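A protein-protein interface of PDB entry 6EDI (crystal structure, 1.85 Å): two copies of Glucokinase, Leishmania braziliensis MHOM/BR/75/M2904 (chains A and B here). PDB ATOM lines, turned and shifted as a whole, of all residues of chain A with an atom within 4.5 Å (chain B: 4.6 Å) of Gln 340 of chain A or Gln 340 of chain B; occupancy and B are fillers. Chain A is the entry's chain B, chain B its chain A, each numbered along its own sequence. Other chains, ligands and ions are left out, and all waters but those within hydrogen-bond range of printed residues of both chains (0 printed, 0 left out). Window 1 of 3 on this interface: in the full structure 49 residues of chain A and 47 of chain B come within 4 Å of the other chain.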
ATOM      1  N   LEU A 233      10.524 -19.181  -7.087  1.00  0.00           N
ATOM      2  CA  LEU A 233      10.172 -18.659  -5.769  1.00  0.00           C
ATOM      3  C   LEU A 233       9.387 -19.676  -4.946  1.00  0.00           C
ATOM      4  O   LEU A 233       8.874 -20.671  -5.470  1.00  0.00           O
ATOM      5  CB  LEU A 233       9.339 -17.367  -5.889  1.00  0.00           C
ATOM      6  CG  LEU A 233       9.906 -16.166  -6.639  1.00  0.00           C
ATOM      7  CD1 LEU A 233       8.835 -15.128  -6.946  1.00  0.00           C
ATOM      8  CD2 LEU A 233      11.050 -15.571  -5.843  1.00  0.00           C
ATOM      9  N   GLU A 234       9.275 -19.409  -3.653  1.00  0.00           N
ATOM     10  CA  GLU A 234       8.424 -20.193  -2.772  1.00  0.00           C
ATOM     11  C   GLU A 234       7.438 -19.307  -2.027  1.00  0.00           C
ATOM     12  O   GLU A 234       7.275 -19.452  -0.814  1.00  0.00           O
ATOM     13  CB  GLU A 234       9.255 -20.985  -1.750  1.00  0.00           C
ATOM     14  CG  GLU A 234      10.349 -21.871  -2.350  1.00  0.00           C
ATOM     15  CD  GLU A 234       9.806 -23.060  -3.117  1.00  0.00           C
ATOM     16  OE1 GLU A 234       8.630 -23.407  -2.926  1.00  0.00           O
ATOM     17  OE2 GLU A 234      10.563 -23.652  -3.905  1.00  0.00           O
ATOM     18  N   CYS A 235       6.762 -18.408  -2.741  1.00  0.00           N
ATOM     19  CA  CYS A 235       5.850 -17.483  -2.088  1.00  0.00           C
ATOM     20  C   CYS A 235       4.652 -18.173  -1.467  1.00  0.00           C
ATOM     21  O   CYS A 235       4.029 -17.635  -0.554  1.00  0.00           O
ATOM     22  CB  CYS A 235       5.372 -16.385  -3.053  1.00  0.00           C
ATOM     23  SG  CYS A 235       6.704 -15.313  -3.630  1.00  0.00           S
ATOM     24  N   LEU A 238       5.145 -18.496   2.237  1.00  0.00           N
ATOM     25  CA  LEU A 238       5.079 -17.314   3.112  1.00  0.00           C
ATOM     26  C   LEU A 238       3.954 -17.533   4.122  1.00  0.00           C
ATOM     27  O   LEU A 238       2.900 -18.048   3.761  1.00  0.00           O
ATOM     28  CB  LEU A 238       4.805 -16.066   2.275  1.00  0.00           C
ATOM     29  CG  LEU A 238       4.357 -14.723   2.867  1.00  0.00           C
ATOM     30  CD1 LEU A 238       5.438 -14.103   3.732  1.00  0.00           C
ATOM     31  CD2 LEU A 238       3.949 -13.750   1.755  1.00  0.00           C
ATOM     32  N   GLU A 336       0.610  -9.471  -1.015  1.00  0.00           N
ATOM     33  CA  GLU A 336       1.967  -9.451  -0.492  1.00  0.00           C
ATOM     34  C   GLU A 336       3.018  -9.582  -1.582  1.00  0.00           C
ATOM     35  O   GLU A 336       4.064  -8.941  -1.510  1.00  0.00           O
ATOM     36  CB  GLU A 336       2.169 -10.561   0.541  1.00  0.00           C
ATOM     37  CG  GLU A 336       1.106 -10.588   1.622  1.00  0.00           C
ATOM     38  CD  GLU A 336       1.099  -9.344   2.481  1.00  0.00           C
ATOM     39  OE1 GLU A 336       2.122  -8.631   2.554  1.00  0.00           O
ATOM     40  OE2 GLU A 336       0.053  -9.090   3.097  1.00  0.00           O
ATOM     41  N   THR A 337       2.769 -10.412  -2.589  1.00  0.00           N
ATOM     42  CA  THR A 337       3.757 -10.535  -3.659  1.00  0.00           C
ATOM     43  C   THR A 337       3.730  -9.298  -4.524  1.00  0.00           C
ATOM     44  O   THR A 337       4.763  -8.869  -5.026  1.00  0.00           O
ATOM     45  CB  THR A 337       3.546 -11.784  -4.549  1.00  0.00           C
ATOM     46  OG1 THR A 337       2.241 -11.744  -5.147  1.00  0.00           O
ATOM     47  CG2 THR A 337       3.693 -13.074  -3.708  1.00  0.00           C
ATOM     48  N   THR A 338       2.543  -8.715  -4.690  1.00  0.00           N
ATOM     49  CA  THR A 338       2.435  -7.505  -5.501  1.00  0.00           C
ATOM     50  C   THR A 338       3.202  -6.370  -4.826  1.00  0.00           C
ATOM     51  O   THR A 338       3.940  -5.656  -5.491  1.00  0.00           O
ATOM     52  CB  THR A 338       0.972  -7.084  -5.734  1.00  0.00           C
ATOM     53  OG1 THR A 338       0.306  -8.125  -6.461  1.00  0.00           O
ATOM     54  CG2 THR A 338       0.875  -5.772  -6.529  1.00  0.00           C
ATOM     55  N   MET A 339       3.036  -6.209  -3.513  1.00  0.00           N
ATOM     56  CA  MET A 339       3.796  -5.179  -2.806  1.00  0.00           C
ATOM     57  C   MET A 339       5.301  -5.448  -2.865  1.00  0.00           C
ATOM     58  O   MET A 339       6.089  -4.542  -3.156  1.00  0.00           O
ATOM     59  CB  MET A 339       3.353  -5.056  -1.355  1.00  0.00           C
ATOM     60  CG  MET A 339       4.075  -3.933  -0.602  1.00  0.00           C
ATOM     61  SD  MET A 339       3.690  -2.315  -1.293  1.00  0.00           S
ATOM     62  CE  MET A 339       5.328  -1.654  -1.614  1.00  0.00           C
ATOM     63  N   GLN A 340       5.713  -6.681  -2.577  1.00  0.00           N
ATOM     64  CA  GLN A 340       7.152  -6.958  -2.468  1.00  0.00           C
ATOM     65  C   GLN A 340       7.893  -6.725  -3.766  1.00  0.00           C
ATOM     66  O   GLN A 340       9.013  -6.216  -3.759  1.00  0.00           O
ATOM     67  CB  GLN A 340       7.420  -8.401  -2.023  1.00  0.00           C
ATOM     68  CG  GLN A 340       7.086  -8.705  -0.587  1.00  0.00           C
ATOM     69  CD  GLN A 340       7.344 -10.166  -0.268  1.00  0.00           C
ATOM     70  OE1 GLN A 340       6.430 -10.995  -0.321  1.00  0.00           O
ATOM     71  NE2 GLN A 340       8.592 -10.493   0.026  1.00  0.00           N
ATOM     72  N   PHE A 341       7.281  -7.136  -4.878  1.00  0.00           N
ATOM     73  CA  PHE A 341       7.947  -7.082  -6.165  1.00  0.00           C
ATOM     74  C   PHE A 341       7.477  -5.905  -7.008  1.00  0.00           C
ATOM     75  O   PHE A 341       8.075  -5.627  -8.048  1.00  0.00           O
ATOM     76  CB  PHE A 341       7.729  -8.405  -6.943  1.00  0.00           C
ATOM     77  CG  PHE A 341       8.225  -9.613  -6.213  1.00  0.00           C
ATOM     78  CD1 PHE A 341       9.587  -9.809  -6.018  1.00  0.00           C
ATOM     79  CD2 PHE A 341       7.328 -10.545  -5.692  1.00  0.00           C
ATOM     80  CE1 PHE A 341      10.056 -10.936  -5.325  1.00  0.00           C
ATOM     81  CE2 PHE A 341       7.781 -11.663  -5.004  1.00  0.00           C
ATOM     82  CZ  PHE A 341       9.152 -11.850  -4.808  1.00  0.00           C
ATOM     83  N   LEU A 342       6.422  -5.215  -6.563  1.00  0.00           N
ATOM     84  CA  LEU A 342       5.788  -4.152  -7.369  1.00  0.00           C
ATOM     85  C   LEU A 342       5.765  -4.450  -8.875  1.00  0.00           C
ATOM     86  O   LEU A 342       6.334  -3.692  -9.669  1.00  0.00           O
ATOM     87  CB  LEU A 342       6.479  -2.817  -7.114  1.00  0.00           C
ATOM     88  CG  LEU A 342       6.327  -2.289  -5.685  1.00  0.00           C
ATOM     89  CD1 LEU A 342       7.171  -1.052  -5.482  1.00  0.00           C
ATOM     90  CD2 LEU A 342       4.892  -1.995  -5.359  1.00  0.00           C
ATOM     91  N   LEU B 233      13.859  -4.701  -3.922  1.00  0.00           N
ATOM     92  CA  LEU B 233      12.661  -5.298  -3.316  1.00  0.00           C
ATOM     93  C   LEU B 233      11.942  -4.357  -2.342  1.00  0.00           C
ATOM     94  O   LEU B 233      12.498  -3.343  -1.921  1.00  0.00           O
ATOM     95  CB  LEU B 233      13.038  -6.580  -2.575  1.00  0.00           C
ATOM     96  CG  LEU B 233      13.611  -7.749  -3.373  1.00  0.00           C
ATOM     97  CD1 LEU B 233      14.054  -8.850  -2.436  1.00  0.00           C
ATOM     98  CD2 LEU B 233      12.571  -8.279  -4.351  1.00  0.00           C
ATOM     99  N   GLU B 234      10.719  -4.719  -1.965  1.00  0.00           N
ATOM    100  CA  GLU B 234       9.992  -4.008  -0.904  1.00  0.00           C
ATOM    101  C   GLU B 234       9.504  -4.963   0.195  1.00  0.00           C
ATOM    102  O   GLU B 234       8.345  -4.911   0.612  1.00  0.00           O
ATOM    103  CB  GLU B 234       8.795  -3.216  -1.470  1.00  0.00           C
ATOM    104  CG  GLU B 234       9.127  -2.249  -2.607  1.00  0.00           C
ATOM    105  CD  GLU B 234      10.057  -1.116  -2.176  1.00  0.00           C
ATOM    106  OE1 GLU B 234      10.182  -0.835  -0.960  1.00  0.00           O
ATOM    107  OE2 GLU B 234      10.664  -0.495  -3.065  1.00  0.00           O
ATOM    108  N   CYS B 235      10.401  -5.813   0.678  1.00  0.00           N
ATOM    109  CA  CYS B 235      10.060  -6.814   1.679  1.00  0.00           C
ATOM    110  C   CYS B 235       9.710  -6.210   3.040  1.00  0.00           C
ATOM    111  O   CYS B 235       8.933  -6.794   3.803  1.00  0.00           O
ATOM    112  CB  CYS B 235      11.196  -7.846   1.820  1.00  0.00           C
ATOM    113  SG  CYS B 235      11.467  -8.877   0.335  1.00  0.00           S
ATOM    114  N   LEU B 238       6.000  -5.916   3.329  1.00  0.00           N
ATOM    115  CA  LEU B 238       5.181  -7.107   3.489  1.00  0.00           C
ATOM    116  C   LEU B 238       4.451  -7.019   4.839  1.00  0.00           C
ATOM    117  O   LEU B 238       5.035  -6.595   5.845  1.00  0.00           O
ATOM    118  CB  LEU B 238       6.070  -8.353   3.379  1.00  0.00           C
ATOM    119  CG  LEU B 238       5.784  -9.717   3.996  1.00  0.00           C
ATOM    120  CD1 LEU B 238       4.672 -10.463   3.287  1.00  0.00           C
ATOM    121  CD2 LEU B 238       7.085 -10.547   3.969  1.00  0.00           C
ATOM    122  N   GLU B 336      10.347 -15.021   6.789  1.00  0.00           N
ATOM    123  CA  GLU B 336       9.569 -14.962   5.549  1.00  0.00           C
ATOM    124  C   GLU B 336      10.438 -14.843   4.287  1.00  0.00           C
ATOM    125  O   GLU B 336      10.191 -15.523   3.292  1.00  0.00           O
ATOM    126  CB  GLU B 336       8.537 -13.823   5.589  1.00  0.00           C
ATOM    127  CG  GLU B 336       7.474 -13.931   6.693  1.00  0.00           C
ATOM    128  CD  GLU B 336       6.874 -15.325   6.863  1.00  0.00           C
ATOM    129  OE1 GLU B 336       6.729 -16.090   5.879  1.00  0.00           O
ATOM    130  OE2 GLU B 336       6.523 -15.660   8.010  1.00  0.00           O
ATOM    131  N   THR B 337      11.453 -13.986   4.311  1.00  0.00           N
ATOM    132  CA  THR B 337      12.270 -13.797   3.108  1.00  0.00           C
ATOM    133  C   THR B 337      13.136 -15.023   2.839  1.00  0.00           C
ATOM    134  O   THR B 337      13.353 -15.402   1.681  1.00  0.00           O
ATOM    135  CB  THR B 337      13.126 -12.504   3.172  1.00  0.00           C
ATOM    136  OG1 THR B 337      14.074 -12.589   4.248  1.00  0.00           O
ATOM    137  CG2 THR B 337      12.221 -11.289   3.387  1.00  0.00           C
ATOM    138  N   THR B 338      13.591 -15.662   3.919  1.00  0.00           N
ATOM    139  CA  THR B 338      14.425 -16.850   3.833  1.00  0.00           C
ATOM    140  C   THR B 338      13.612 -17.984   3.234  1.00  0.00           C
ATOM    141  O   THR B 338      14.093 -18.727   2.364  1.00  0.00           O
ATOM    142  CB  THR B 338      14.966 -17.255   5.211  1.00  0.00           C
ATOM    143  OG1 THR B 338      15.795 -16.193   5.723  1.00  0.00           O
ATOM    144  CG2 THR B 338      15.768 -18.540   5.139  1.00  0.00           C
ATOM    145  N   MET B 339      12.373 -18.139   3.686  1.00  0.00           N
ATOM    146  CA  MET B 339      11.524 -19.141   3.052  1.00  0.00           C
ATOM    147  C   MET B 339      11.230 -18.818   1.575  1.00  0.00           C
ATOM    148  O   MET B 339      11.328 -19.691   0.730  1.00  0.00           O
ATOM    149  CB  MET B 339      10.220 -19.334   3.843  1.00  0.00           C
ATOM    150  CG  MET B 339       9.332 -20.446   3.267  1.00  0.00           C
ATOM    151  SD  MET B 339      10.086 -22.073   3.383  1.00  0.00           S
ATOM    152  CE  MET B 339      10.139 -22.536   1.659  1.00  0.00           C
ATOM    153  N   GLN B 340      10.873 -17.581   1.239  1.00  0.00           N
ATOM    154  CA  GLN B 340      10.466 -17.337  -0.151  1.00  0.00           C
ATOM    155  C   GLN B 340      11.597 -17.501  -1.143  1.00  0.00           C
ATOM    156  O   GLN B 340      11.394 -18.003  -2.244  1.00  0.00           O
ATOM    157  CB  GLN B 340       9.904 -15.935  -0.331  1.00  0.00           C
ATOM    158  CG  GLN B 340       8.620 -15.667   0.403  1.00  0.00           C
ATOM    159  CD  GLN B 340       8.262 -14.217   0.284  1.00  0.00           C
ATOM    160  OE1 GLN B 340       8.632 -13.401   1.138  1.00  0.00           O
ATOM    161  NE2 GLN B 340       7.588 -13.867  -0.808  1.00  0.00           N
ATOM    162  N   PHE B 341      12.782 -17.052  -0.759  1.00  0.00           N
ATOM    163  CA  PHE B 341      13.915 -17.042  -1.670  1.00  0.00           C
ATOM    164  C   PHE B 341      14.918 -18.195  -1.503  1.00  0.00           C
ATOM    165  O   PHE B 341      15.827 -18.373  -2.354  1.00  0.00           O
ATOM    166  CB  PHE B 341      14.651 -15.707  -1.492  1.00  0.00           C
ATOM    167  CG  PHE B 341      13.813 -14.507  -1.811  1.00  0.00           C
ATOM    168  CD1 PHE B 341      13.266 -14.353  -3.080  1.00  0.00           C
ATOM    169  CD2 PHE B 341      13.603 -13.506  -0.855  1.00  0.00           C
ATOM    170  CE1 PHE B 341      12.514 -13.231  -3.411  1.00  0.00           C
ATOM    171  CE2 PHE B 341      12.840 -12.371  -1.162  1.00  0.00           C
ATOM    172  CZ  PHE B 341      12.283 -12.234  -2.439  1.00  0.00           C
ATOM    173  N   LEU B 342      14.778 -18.953  -0.411  1.00  0.00           N
ATOM    174  CA  LEU B 342      15.742 -20.022  -0.034  1.00  0.00           C
ATOM    175  C   LEU B 342      17.210 -19.637  -0.306  1.00  0.00           C
ATOM    176  O   LEU B 342      17.920 -20.300  -1.066  1.00  0.00           O
ATOM    177  CB  LEU B 342      15.367 -21.375  -0.668  1.00  0.00           C
ATOM    178  CG  LEU B 342      14.023 -21.963  -0.253  1.00  0.00           C
ATOM    179  CD1 LEU B 342      13.689 -23.235  -1.057  1.00  0.00           C
ATOM    180  CD2 LEU B 342      13.996 -22.272   1.246  1.00  0.00           C
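Of the 11 printed residues of chain A, 9 touch a printed residue of chain B.
Hydrophobic or aromatic side chains of chain A within 4 Å of the printed part of chain B: Leu 233, Leu 238, Met 339, Phe 341 and Leu 342.
Among the printed residues, 17 pairs touch across the chains.
Among the printed residues, no Asp or Glu carboxylate lies within 4 Å of a Lys or Arg side-chain nitrogen of the other chain.
OE1 of Gln 340 of chain A lies close to O of Glu 336 of chain A (3.4 Å).
The backbone carbonyl oxygen (O) of Glu 336 of chain B sits close to the side-chain amide oxygen (OE1) of Gln 340 of chain B (3.4 Å).
Of the printed residues of chain B, Leu 238 of chain A touches Leu 238 (3.7 Å) and Glu 336 (3.2 Å).
Of the printed residues of chain B, Glu 336 of chain A touches Leu 238 (3.2 Å).
Thr 338 of chain A touches none of the printed residues of chain B.
Gln 340 of chain A touches just these residues of chain B: Leu 233, Glu 234, Cys 235 and Gln 340.
Of the printed residues of chain B, Phe 341 of chain A touches Leu 233 and Phe 341.
Of the printed residues of chain A, Leu 238 of chain B touches Leu 238 and Glu 336.
Thr 338 of chain B touches none of the printed residues of chain A.
Printed residues of chain A within 4 Å of Gln 340 of chain B: Leu 233 (3.8 Å), Glu 234 (2.9 Å), Cys 235 (3.3 Å) and Gln 340 (3.1 Å).
The nearest residue of chain B that does not touch Gln 340 of chain A is Leu 238 of chain B (4.05 Å).
The nearest residue of chain A that does not touch Gln 340 of chain B is Leu 238 of chain A (4.2 Å).
The nearest printed residue of chain B that does not touch Met 339 of chain A is Leu 238 of chain B (4.8 Å).
The backbone NH of Glu 234 of chain B sits at hydrogen-bond distance from the backbone carbonyl oxygen of Gln 340 of chain A, at 2.9 Å.
O of Gln 340 of chain B is in hydrogen-bond range of N of Glu 234 of chain A (2.9 Å).
NE2 of Gln 340 of chain A sits at hydrogen-bond distance from SG of Cys 235 of chain B (3.3 Å).
The side-chain sulfur of Cys 235 of chain A lies within hydrogen-bond range of the side-chain amide nitrogen of Gln 340 of chain B, at 3.3 Å.
The side-chain amide oxygen (OE1) of Gln 340 of chain B lies within hydrogen-bond range of the side-chain amide nitrogen (NE2) of Gln 340 of chain A (3.1 Å).
Glu 234 of chain A touches Met 339 of chain B, and with the chains exchanged Met 339 of chain A touches Glu 234 of chain B.
Glu 234 of chain A touches Leu 342 of chain B, and with the chains exchanged Leu 342 of chain A touches Glu 234 of chain B.
Leu 238 of chain A touches its own counterpart, Leu 238 of chain B.
Phe 341 of chain A touches its own counterpart, Phe 341 of chain B.
Positions printed for both chains: 233, 234, 235, 238, 336, 337, 338, 339, 340, 341 and 342.
Leu 233 of chain A touches Gln 340 of chain B (C to O, 3.8 Å).
CE1 of Phe 341 of chain B touches CD2 of Leu 233 of chain A, at 3.7 Å.
Glu 234 of chain A touches Met 339 of chain B (CB to O, 3.5 Å).
Glu 234 of chain A touches Leu 342 of chain B.
Glu 336 of chain B touches Leu 238 of chain A (OE1 to CD1, 3.2 Å).
CD1 of Leu 238 of chain B touches OE1 of Glu 336 of chain A (3.2 Å).
Glu 234 of chain B touches Met 339 of chain A.
Leu 233 of chain B touches Gln 340 of chain A (C to O, 3.7 Å).
CE1 of Phe 341 of chain B touches CE1 of Phe 341 of chain A, at 3.9 Å.
CG of Glu 234 of chain B touches CD1 of Leu 342 of chain A (3.7 Å).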
